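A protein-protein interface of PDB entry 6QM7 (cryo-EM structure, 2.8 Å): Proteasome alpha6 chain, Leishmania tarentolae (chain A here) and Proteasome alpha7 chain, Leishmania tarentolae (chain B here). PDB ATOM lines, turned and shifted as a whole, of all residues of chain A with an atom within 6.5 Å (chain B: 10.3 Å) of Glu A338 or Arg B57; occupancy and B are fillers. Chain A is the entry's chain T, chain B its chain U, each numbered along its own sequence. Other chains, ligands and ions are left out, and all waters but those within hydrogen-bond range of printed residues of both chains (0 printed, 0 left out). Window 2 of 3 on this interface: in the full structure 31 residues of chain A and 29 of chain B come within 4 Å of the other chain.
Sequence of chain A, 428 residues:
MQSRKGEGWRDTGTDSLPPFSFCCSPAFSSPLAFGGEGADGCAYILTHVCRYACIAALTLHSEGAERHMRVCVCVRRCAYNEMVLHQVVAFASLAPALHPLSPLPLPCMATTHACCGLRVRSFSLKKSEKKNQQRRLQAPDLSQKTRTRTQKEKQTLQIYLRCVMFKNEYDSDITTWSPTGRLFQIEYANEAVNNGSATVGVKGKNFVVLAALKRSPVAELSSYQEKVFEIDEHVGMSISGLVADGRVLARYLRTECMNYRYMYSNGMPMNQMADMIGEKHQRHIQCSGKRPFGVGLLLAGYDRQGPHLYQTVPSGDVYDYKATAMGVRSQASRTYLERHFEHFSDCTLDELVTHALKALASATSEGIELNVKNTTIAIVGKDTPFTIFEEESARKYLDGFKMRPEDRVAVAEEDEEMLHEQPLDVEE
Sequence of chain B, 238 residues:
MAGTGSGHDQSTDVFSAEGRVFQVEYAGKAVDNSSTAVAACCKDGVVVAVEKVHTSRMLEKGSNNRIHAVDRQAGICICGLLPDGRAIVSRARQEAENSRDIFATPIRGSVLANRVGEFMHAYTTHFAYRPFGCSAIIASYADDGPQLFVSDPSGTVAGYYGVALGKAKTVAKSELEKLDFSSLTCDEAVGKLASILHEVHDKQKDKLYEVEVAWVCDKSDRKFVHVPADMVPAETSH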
ATOM      1  N   TYR A 321     -11.526 -33.877  33.680  1.00  0.00           N
ATOM      2  CA  TYR A 321     -11.994 -32.475  33.595  1.00  0.00           C
ATOM      3  C   TYR A 321     -10.902 -31.548  34.120  1.00  0.00           C
ATOM      4  O   TYR A 321     -10.138 -31.987  34.991  1.00  0.00           O
ATOM      5  CB  TYR A 321     -13.280 -32.329  34.396  1.00  0.00           C
ATOM      6  CG  TYR A 321     -14.558 -32.442  33.607  1.00  0.00           C
ATOM      7  CD1 TYR A 321     -14.907 -31.462  32.696  1.00  0.00           C
ATOM      8  CD2 TYR A 321     -15.472 -33.464  33.835  1.00  0.00           C
ATOM      9  CE1 TYR A 321     -16.103 -31.516  31.998  1.00  0.00           C
ATOM     10  CE2 TYR A 321     -16.678 -33.527  33.150  1.00  0.00           C
ATOM     11  CZ  TYR A 321     -16.994 -32.550  32.223  1.00  0.00           C
ATOM     12  OH  TYR A 321     -18.162 -32.598  31.511  1.00  0.00           O
ATOM     13  N   LYS A 322     -10.810 -30.335  33.566  1.00  0.00           N
ATOM     14  CA  LYS A 322     -10.020 -29.203  34.122  1.00  0.00           C
ATOM     15  C   LYS A 322     -10.849 -28.564  35.235  1.00  0.00           C
ATOM     16  O   LYS A 322     -10.284 -28.189  36.277  1.00  0.00           O
ATOM     17  CB  LYS A 322      -9.690 -28.144  33.063  1.00  0.00           C
ATOM     18  CG  LYS A 322      -8.611 -28.538  32.065  1.00  0.00           C
ATOM     19  CD  LYS A 322      -8.017 -27.355  31.314  1.00  0.00           C
ATOM     20  CE  LYS A 322      -7.255 -27.743  30.063  1.00  0.00           C
ATOM     21  NZ  LYS A 322      -8.180 -28.150  28.979  1.00  0.00           N
ATOM     22  N   GLN A 331     -25.589 -25.935  35.684  1.00  0.00           N
ATOM     23  CA  GLN A 331     -25.337 -25.310  34.356  1.00  0.00           C
ATOM     24  C   GLN A 331     -24.861 -23.867  34.573  1.00  0.00           C
ATOM     25  O   GLN A 331     -24.070 -23.388  33.738  1.00  0.00           O
ATOM     26  CB  GLN A 331     -26.556 -25.358  33.430  1.00  0.00           C
ATOM     27  CG  GLN A 331     -26.261 -25.934  32.044  1.00  0.00           C
ATOM     28  CD  GLN A 331     -25.258 -25.161  31.214  1.00  0.00           C
ATOM     29  OE1 GLN A 331     -25.601 -24.571  30.193  1.00  0.00           O
ATOM     30  NE2 GLN A 331     -23.998 -25.173  31.622  1.00  0.00           N
ATOM     31  N   SER A 333     -23.030 -22.896  37.322  1.00  0.00           N
ATOM     32  CA  SER A 333     -21.637 -23.122  37.798  1.00  0.00           C
ATOM     33  C   SER A 333     -20.721 -23.356  36.599  1.00  0.00           C
ATOM     34  O   SER A 333     -19.668 -22.709  36.540  1.00  0.00           O
ATOM     35  CB  SER A 333     -21.529 -24.271  38.765  1.00  0.00           C
ATOM     36  OG  SER A 333     -21.959 -23.890  40.060  1.00  0.00           O
ATOM     37  N   ARG A 334     -21.116 -24.248  35.687  1.00  0.00           N
ATOM     38  CA  ARG A 334     -20.316 -24.606  34.485  1.00  0.00           C
ATOM     39  C   ARG A 334     -20.179 -23.379  33.580  1.00  0.00           C
ATOM     40  O   ARG A 334     -19.123 -23.254  32.949  1.00  0.00           O
ATOM     41  CB  ARG A 334     -20.908 -25.812  33.743  1.00  0.00           C
ATOM     42  CG  ARG A 334     -20.606 -27.145  34.416  1.00  0.00           C
ATOM     43  CD  ARG A 334     -20.749 -28.361  33.522  1.00  0.00           C
ATOM     44  NE  ARG A 334     -22.083 -28.411  32.933  1.00  0.00           N
ATOM     45  CZ  ARG A 334     -23.210 -28.780  33.557  1.00  0.00           C
ATOM     46  NH1 ARG A 334     -23.208 -29.153  34.832  1.00  0.00           N
ATOM     47  NH2 ARG A 334     -24.353 -28.775  32.886  1.00  0.00           N
ATOM     48  N   THR A 335     -21.182 -22.496  33.542  1.00  0.00           N
ATOM     49  CA  THR A 335     -21.115 -21.220  32.782  1.00  0.00           C
ATOM     50  C   THR A 335     -20.007 -20.360  33.391  1.00  0.00           C
ATOM     51  O   THR A 335     -19.161 -19.884  32.614  1.00  0.00           O
ATOM     52  CB  THR A 335     -22.472 -20.504  32.716  1.00  0.00           C
ATOM     53  OG1 THR A 335     -23.337 -21.278  31.883  1.00  0.00           O
ATOM     54  CG2 THR A 335     -22.378 -19.098  32.163  1.00  0.00           C
ATOM     55  N   TYR A 336     -19.999 -20.186  34.717  1.00  0.00           N
ATOM     56  CA  TYR A 336     -18.964 -19.388  35.429  1.00  0.00           C
ATOM     57  C   TYR A 336     -17.588 -19.993  35.141  1.00  0.00           C
ATOM     58  O   TYR A 336     -16.697 -19.249  34.708  1.00  0.00           O
ATOM     59  CB  TYR A 336     -19.172 -19.302  36.943  1.00  0.00           C
ATOM     60  CG  TYR A 336     -17.991 -18.676  37.646  1.00  0.00           C
ATOM     61  CD1 TYR A 336     -17.899 -17.301  37.808  1.00  0.00           C
ATOM     62  CD2 TYR A 336     -16.922 -19.451  38.078  1.00  0.00           C
ATOM     63  CE1 TYR A 336     -16.799 -16.718  38.420  1.00  0.00           C
ATOM     64  CE2 TYR A 336     -15.809 -18.884  38.682  1.00  0.00           C
ATOM     65  CZ  TYR A 336     -15.746 -17.511  38.853  1.00  0.00           C
ATOM     66  OH  TYR A 336     -14.659 -16.951  39.462  1.00  0.00           O
ATOM     67  N   LEU A 337     -17.427 -21.293  35.391  1.00  0.00           N
ATOM     68  CA  LEU A 337     -16.147 -22.021  35.204  1.00  0.00           C
ATOM     69  C   LEU A 337     -15.648 -21.842  33.767  1.00  0.00           C
ATOM     70  O   LEU A 337     -14.439 -21.641  33.613  1.00  0.00           O
ATOM     71  CB  LEU A 337     -16.350 -23.496  35.551  1.00  0.00           C
ATOM     72  CG  LEU A 337     -16.520 -23.805  37.040  1.00  0.00           C
ATOM     73  CD1 LEU A 337     -16.856 -25.271  37.267  1.00  0.00           C
ATOM     74  CD2 LEU A 337     -15.268 -23.426  37.814  1.00  0.00           C
ATOM     75  N   GLU A 338     -16.527 -21.858  32.760  1.00  0.00           N
ATOM     76  CA  GLU A 338     -16.139 -21.734  31.324  1.00  0.00           C
ATOM     77  C   GLU A 338     -15.488 -20.369  31.048  1.00  0.00           C
ATOM     78  O   GLU A 338     -14.662 -20.307  30.121  1.00  0.00           O
ATOM     79  CB  GLU A 338     -17.339 -21.984  30.405  1.00  0.00           C
ATOM     80  CG  GLU A 338     -17.557 -23.462  30.092  1.00  0.00           C
ATOM     81  CD  GLU A 338     -18.990 -23.901  29.808  1.00  0.00           C
ATOM     82  OE1 GLU A 338     -19.335 -25.048  30.181  1.00  0.00           O
ATOM     83  OE2 GLU A 338     -19.760 -23.104  29.221  1.00  0.00           O
ATOM     84  N   ARG A 339     -15.844 -19.319  31.800  1.00  0.00           N
ATOM     85  CA  ARG A 339     -15.262 -17.956  31.647  1.00  0.00           C
ATOM     86  C   ARG A 339     -13.812 -17.933  32.142  1.00  0.00           C
ATOM     87  O   ARG A 339     -13.043 -17.112  31.618  1.00  0.00           O
ATOM     88  CB  ARG A 339     -16.075 -16.898  32.401  1.00  0.00           C
ATOM     89  CG  ARG A 339     -17.361 -16.475  31.699  1.00  0.00           C
ATOM     90  CD  ARG A 339     -17.929 -15.161  32.223  1.00  0.00           C
ATOM     91  NE  ARG A 339     -18.716 -15.313  33.450  1.00  0.00           N
ATOM     92  CZ  ARG A 339     -20.017 -15.632  33.519  1.00  0.00           C
ATOM     93  NH1 ARG A 339     -20.603 -15.731  34.702  1.00  0.00           N
ATOM     94  NH2 ARG A 339     -20.731 -15.860  32.425  1.00  0.00           N
ATOM     95  N   HIS A 340     -13.452 -18.787  33.107  1.00  0.00           N
ATOM     96  CA  HIS A 340     -12.239 -18.630  33.953  1.00  0.00           C
ATOM     97  C   HIS A 340     -11.296 -19.842  33.899  1.00  0.00           C
ATOM     98  O   HIS A 340     -10.138 -19.680  34.330  1.00  0.00           O
ATOM     99  CB  HIS A 340     -12.670 -18.319  35.394  1.00  0.00           C
ATOM    100  CG  HIS A 340     -13.306 -16.977  35.551  1.00  0.00           C
ATOM    101  ND1 HIS A 340     -14.678 -16.802  35.525  1.00  0.00           N
ATOM    102  CD2 HIS A 340     -12.771 -15.750  35.731  1.00  0.00           C
ATOM    103  CE1 HIS A 340     -14.962 -15.525  35.675  1.00  0.00           C
ATOM    104  NE2 HIS A 340     -13.812 -14.860  35.809  1.00  0.00           N
ATOM    105  N   PHE A 341     -11.735 -21.002  33.403  1.00  0.00           N
ATOM    106  CA  PHE A 341     -11.051 -22.306  33.625  1.00  0.00           C
ATOM    107  C   PHE A 341      -9.666 -22.313  32.967  1.00  0.00           C
ATOM    108  O   PHE A 341      -8.795 -23.061  33.450  1.00  0.00           O
ATOM    109  CB  PHE A 341     -11.893 -23.482  33.123  1.00  0.00           C
ATOM    110  CG  PHE A 341     -11.807 -23.736  31.639  1.00  0.00           C
ATOM    111  CD1 PHE A 341     -10.970 -24.725  31.138  1.00  0.00           C
ATOM    112  CD2 PHE A 341     -12.547 -22.980  30.746  1.00  0.00           C
ATOM    113  CE1 PHE A 341     -10.888 -24.957  29.775  1.00  0.00           C
ATOM    114  CE2 PHE A 341     -12.464 -23.215  29.382  1.00  0.00           C
ATOM    115  CZ  PHE A 341     -11.639 -24.206  28.899  1.00  0.00           C
ATOM    116  N   GLU A 342      -9.474 -21.522  31.906  1.00  0.00           N
ATOM    117  CA  GLU A 342      -8.191 -21.428  31.155  1.00  0.00           C
ATOM    118  C   GLU A 342      -7.069 -20.915  32.071  1.00  0.00           C
ATOM    119  O   GLU A 342      -5.909 -21.254  31.791  1.00  0.00           O
ATOM    120  CB  GLU A 342      -8.355 -20.530  29.924  1.00  0.00           C
ATOM    121  CG  GLU A 342      -9.242 -21.126  28.834  1.00  0.00           C
ATOM    122  CD  GLU A 342      -8.664 -22.307  28.060  1.00  0.00           C
ATOM    123  OE1 GLU A 342      -7.483 -22.657  28.284  1.00  0.00           O
ATOM    124  OE2 GLU A 342      -9.399 -22.878  27.225  1.00  0.00           O
ATOM    125  N   VAL B  53     -16.573 -36.521  20.203  1.00  0.00           N
ATOM    126  CA  VAL B  53     -17.449 -35.342  20.434  1.00  0.00           C
ATOM    127  C   VAL B  53     -17.423 -35.047  21.934  1.00  0.00           C
ATOM    128  O   VAL B  53     -17.959 -35.855  22.705  1.00  0.00           O
ATOM    129  CB  VAL B  53     -18.875 -35.578  19.909  1.00  0.00           C
ATOM    130  CG1 VAL B  53     -19.796 -34.400  20.227  1.00  0.00           C
ATOM    131  CG2 VAL B  53     -18.847 -35.880  18.416  1.00  0.00           C
ATOM    132  N   HIS B  54     -16.798 -33.933  22.306  1.00  0.00           N
ATOM    133  CA  HIS B  54     -16.721 -33.404  23.686  1.00  0.00           C
ATOM    134  C   HIS B  54     -17.990 -32.608  23.984  1.00  0.00           C
ATOM    135  O   HIS B  54     -18.331 -31.716  23.192  1.00  0.00           O
ATOM    136  CB  HIS B  54     -15.460 -32.550  23.839  1.00  0.00           C
ATOM    137  CG  HIS B  54     -14.198 -33.341  23.874  1.00  0.00           C
ATOM    138  ND1 HIS B  54     -12.976 -32.780  23.577  1.00  0.00           N
ATOM    139  CD2 HIS B  54     -13.960 -34.635  24.193  1.00  0.00           C
ATOM    140  CE1 HIS B  54     -12.036 -33.690  23.725  1.00  0.00           C
ATOM    141  NE2 HIS B  54     -12.613 -34.842  24.096  1.00  0.00           N
ATOM    142  N   THR B  55     -18.659 -32.931  25.088  1.00  0.00           N
ATOM    143  CA  THR B  55     -19.877 -32.235  25.582  1.00  0.00           C
ATOM    144  C   THR B  55     -19.501 -30.863  26.169  1.00  0.00           C
ATOM    145  O   THR B  55     -20.379 -29.986  26.178  1.00  0.00           O
ATOM    146  CB  THR B  55     -20.640 -33.138  26.565  1.00  0.00           C
ATOM    147  OG1 THR B  55     -21.852 -32.466  26.915  1.00  0.00           O
ATOM    148  CG2 THR B  55     -19.856 -33.505  27.814  1.00  0.00           C
ATOM    149  N   SER B  56     -18.254 -30.689  26.632  1.00  0.00           N
ATOM    150  CA  SER B  56     -17.775 -29.531  27.437  1.00  0.00           C
ATOM    151  C   SER B  56     -16.424 -29.025  26.924  1.00  0.00           C
ATOM    152  O   SER B  56     -15.592 -29.855  26.499  1.00  0.00           O
ATOM    153  CB  SER B  56     -17.678 -29.906  28.902  1.00  0.00           C
ATOM    154  OG  SER B  56     -17.115 -28.853  29.681  1.00  0.00           O
ATOM    155  N   ARG B  57     -16.191 -27.715  27.065  1.00  0.00           N
ATOM    156  CA  ARG B  57     -14.955 -27.003  26.632  1.00  0.00           C
ATOM    157  C   ARG B  57     -13.804 -27.318  27.590  1.00  0.00           C
ATOM    158  O   ARG B  57     -12.644 -27.069  27.216  1.00  0.00           O
ATOM    159  CB  ARG B  57     -15.169 -25.484  26.609  1.00  0.00           C
ATOM    160  CG  ARG B  57     -16.514 -25.025  26.051  1.00  0.00           C
ATOM    161  CD  ARG B  57     -16.497 -23.686  25.328  1.00  0.00           C
ATOM    162  NE  ARG B  57     -15.976 -22.614  26.172  1.00  0.00           N
ATOM    163  CZ  ARG B  57     -14.715 -22.158  26.190  1.00  0.00           C
ATOM    164  NH1 ARG B  57     -13.779 -22.659  25.394  1.00  0.00           N
ATOM    165  NH2 ARG B  57     -14.395 -21.179  27.019  1.00  0.00           N
ATOM    166  N   MET B  58     -14.128 -27.836  28.780  1.00  0.00           N
ATOM    167  CA  MET B  58     -13.241 -27.882  29.969  1.00  0.00           C
ATOM    168  C   MET B  58     -12.735 -29.302  30.227  1.00  0.00           C
ATOM    169  O   MET B  58     -12.240 -29.547  31.339  1.00  0.00           O
ATOM    170  CB  MET B  58     -14.005 -27.407  31.208  1.00  0.00           C
ATOM    171  CG  MET B  58     -14.736 -26.099  31.002  1.00  0.00           C
ATOM    172  SD  MET B  58     -15.261 -25.405  32.578  1.00  0.00           S
ATOM    173  CE  MET B  58     -16.667 -26.447  32.964  1.00  0.00           C
ATOM    174  N   LEU B  59     -12.851 -30.205  29.257  1.00  0.00           N
ATOM    175  CA  LEU B  59     -12.286 -31.570  29.384  1.00  0.00           C
ATOM    176  C   LEU B  59     -10.775 -31.481  29.204  1.00  0.00           C
ATOM    177  O   LEU B  59     -10.327 -30.591  28.468  1.00  0.00           O
ATOM    178  CB  LEU B  59     -12.923 -32.491  28.339  1.00  0.00           C
ATOM    179  CG  LEU B  59     -14.361 -32.921  28.631  1.00  0.00           C
ATOM    180  CD1 LEU B  59     -14.972 -33.616  27.428  1.00  0.00           C
ATOM    181  CD2 LEU B  59     -14.432 -33.835  29.838  1.00  0.00           C
ATOM    182  N   GLU B  60     -10.029 -32.361  29.875  1.00  0.00           N
ATOM    183  CA  GLU B  60      -8.580 -32.585  29.615  1.00  0.00           C
ATOM    184  C   GLU B  60      -8.411 -33.238  28.236  1.00  0.00           C
ATOM    185  O   GLU B  60      -9.360 -33.901  27.765  1.00  0.00           O
ATOM    186  CB  GLU B  60      -7.949 -33.447  30.712  1.00  0.00           C
ATOM    187  CG  GLU B  60      -7.440 -32.640  31.889  1.00  0.00           C
ATOM    188  CD  GLU B  60      -6.219 -31.772  31.600  1.00  0.00           C
ATOM    189  OE1 GLU B  60      -6.195 -30.605  32.051  1.00  0.00           O
ATOM    190  OE2 GLU B  60      -5.283 -32.268  30.935  1.00  0.00           O
ATOM    191  N   LYS B  61      -7.253 -33.034  27.601  1.00  0.00           N
ATOM    192  CA  LYS B  61      -6.823 -33.805  26.400  1.00  0.00           C
ATOM    193  C   LYS B  61      -6.589 -35.256  26.835  1.00  0.00           C
ATOM    194  O   LYS B  61      -5.861 -35.459  27.828  1.00  0.00           O
ATOM    195  CB  LYS B  61      -5.561 -33.212  25.763  1.00  0.00           C
ATOM    196  CG  LYS B  61      -5.810 -32.204  24.646  1.00  0.00           C
ATOM    197  CD  LYS B  61      -6.661 -31.017  25.055  1.00  0.00           C
ATOM    198  CE  LYS B  61      -6.573 -29.867  24.072  1.00  0.00           C
ATOM    199  NZ  LYS B  61      -7.441 -28.733  24.469  1.00  0.00           N
ATOM    200  N   SER B  63      -9.286 -37.236  27.589  1.00  0.00           N
ATOM    201  CA  SER B  63     -10.557 -37.592  28.273  1.00  0.00           C
ATOM    202  C   SER B  63     -11.437 -38.394  27.325  1.00  0.00           C
ATOM    203  O   SER B  63     -11.556 -37.985  26.165  1.00  0.00           O
ATOM    204  CB  SER B  63     -11.318 -36.385  28.748  1.00  0.00           C
ATOM    205  OG  SER B  63     -12.585 -36.775  29.260  1.00  0.00           O
ATOM    206  N   ASN B  64     -12.094 -39.428  27.850  1.00  0.00           N
ATOM    207  CA  ASN B  64     -13.019 -40.309  27.095  1.00  0.00           C
ATOM    208  C   ASN B  64     -12.273 -40.847  25.872  1.00  0.00           C
ATOM    209  O   ASN B  64     -12.864 -40.840  24.767  1.00  0.00           O
ATOM    210  CB  ASN B  64     -14.302 -39.577  26.695  1.00  0.00           C
ATOM    211  CG  ASN B  64     -15.021 -38.937  27.865  1.00  0.00           C
ATOM    212  OD1 ASN B  64     -14.808 -37.763  28.156  1.00  0.00           O
ATOM    213  ND2 ASN B  64     -15.871 -39.699  28.537  1.00  0.00           N
ATOM    214  N   LYS B 207     -19.682 -28.756  18.037  1.00  0.00           N
ATOM    215  CA  LYS B 207     -18.647 -27.685  17.952  1.00  0.00           C
ATOM    216  C   LYS B 207     -17.306 -28.191  18.504  1.00  0.00           C
ATOM    217  O   LYS B 207     -16.276 -28.029  17.815  1.00  0.00           O
ATOM    218  CB  LYS B 207     -19.098 -26.430  18.712  1.00  0.00           C
ATOM    219  CG  LYS B 207     -20.219 -25.636  18.048  1.00  0.00           C
ATOM    220  CD  LYS B 207     -21.337 -25.217  18.992  1.00  0.00           C
ATOM    221  CE  LYS B 207     -22.706 -25.661  18.519  1.00  0.00           C
ATOM    222  NZ  LYS B 207     -23.678 -25.713  19.637  1.00  0.00           N
ATOM    223  N   LEU B 208     -17.332 -28.789  19.697  1.00  0.00           N
ATOM    224  CA  LEU B 208     -16.129 -29.220  20.454  1.00  0.00           C
ATOM    225  C   LEU B 208     -15.855 -30.686  20.122  1.00  0.00           C
ATOM    226  O   LEU B 208     -16.754 -31.514  20.347  1.00  0.00           O
ATOM    227  CB  LEU B 208     -16.385 -29.033  21.953  1.00  0.00           C
ATOM    228  CG  LEU B 208     -16.968 -27.680  22.363  1.00  0.00           C
ATOM    229  CD1 LEU B 208     -17.903 -27.831  23.562  1.00  0.00           C
ATOM    230  CD2 LEU B 208     -15.856 -26.674  22.645  1.00  0.00           C
ATOM    231  N   TYR B 209     -14.677 -30.980  19.570  1.00  0.00           N
ATOM    232  CA  TYR B 209     -14.245 -32.347  19.173  1.00  0.00           C
ATOM    233  C   TYR B 209     -12.736 -32.382  18.925  1.00  0.00           C
ATOM    234  O   TYR B 209     -12.145 -31.341  18.580  1.00  0.00           O
ATOM    235  CB  TYR B 209     -14.982 -32.814  17.911  1.00  0.00           C
ATOM    236  CG  TYR B 209     -14.392 -32.346  16.601  1.00  0.00           C
ATOM    237  CD1 TYR B 209     -13.756 -33.232  15.742  1.00  0.00           C
ATOM    238  CD2 TYR B 209     -14.451 -31.013  16.224  1.00  0.00           C
ATOM    239  CE1 TYR B 209     -13.207 -32.810  14.538  1.00  0.00           C
ATOM    240  CE2 TYR B 209     -13.910 -30.573  15.024  1.00  0.00           C
ATOM    241  CZ  TYR B 209     -13.287 -31.475  14.175  1.00  0.00           C
ATOM    242  OH  TYR B 209     -12.759 -31.042  12.992  1.00  0.00           O
ATOM    243  N   GLU B 210     -12.141 -33.560  19.076  1.00  0.00           N
ATOM    244  CA  GLU B 210     -10.758 -33.841  18.619  1.00  0.00           C
ATOM    245  C   GLU B 210     -10.746 -35.198  17.920  1.00  0.00           C
ATOM    246  O   GLU B 210     -11.690 -35.982  18.135  1.00  0.00           O
ATOM    247  CB  GLU B 210      -9.756 -33.793  19.777  1.00  0.00           C
ATOM    248  CG  GLU B 210     -10.118 -34.681  20.960  1.00  0.00           C
ATOM    249  CD  GLU B 210      -8.960 -35.008  21.900  1.00  0.00           C
ATOM    250  OE1 GLU B 210      -8.923 -34.452  23.026  1.00  0.00           O
ATOM    251  OE2 GLU B 210      -8.094 -35.833  21.507  1.00  0.00           O
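N of Glu A338 lies within hydrogen-bond range of SD of Met B58. NH2 of Arg B57 sits at hydrogen-bond distance from O of Glu A338. The backbone carbonyl oxygen (O) of Leu B59 lies within hydrogen-bond range of the side-chain amino group (NZ) of Lys A322 (3.3 Å). The backbone carbonyl oxygen of Met B58 sits at hydrogen-bond distance from the backbone NH of Lys A322 (2.8 Å).
The backbone NH of Met B58 lies close to the side-chain hydroxyl of Ser B56.
Among the printed residues, merely in contact across the chains: Tyr A321 with Ser B56, Tyr A321 with Met B58, Tyr A321 with Leu B59, Lys A322 with Glu B60, Leu A337 with Met B58, Phe A341 with Arg B57 and Phe A341 with Met B58.
Of chain B, only Arg B57 (3.2 Å) and Met B58 (3.8 Å) come within 4 Å of Glu A338. Arg B57 touches two residues of chain A. No residue of chain B comes within 4 Å of Thr A335. Leu A337 touches just one residue of chain B: Met B58 (3.7 Å). Printed residues of chain A within 4 Å of Leu B59: Tyr A321 (3.6 Å) and Lys A322 (3.3 Å). Printed residues of chain A within 4 Å of Glu B60: Lys A322. Of the printed residues of chain B, Lys A322 touches Met B58 (2.8 Å), Leu B59 (3.3 Å) and Glu B60 (3.2 Å). His B54 touches none of the printed residues of chain A. The nearest printed residue of chain A that does not touch Leu B59 is Phe A341 (5.6 Å).
Of the 13 printed residues of chain A, 5 touch a printed residue of chain B.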
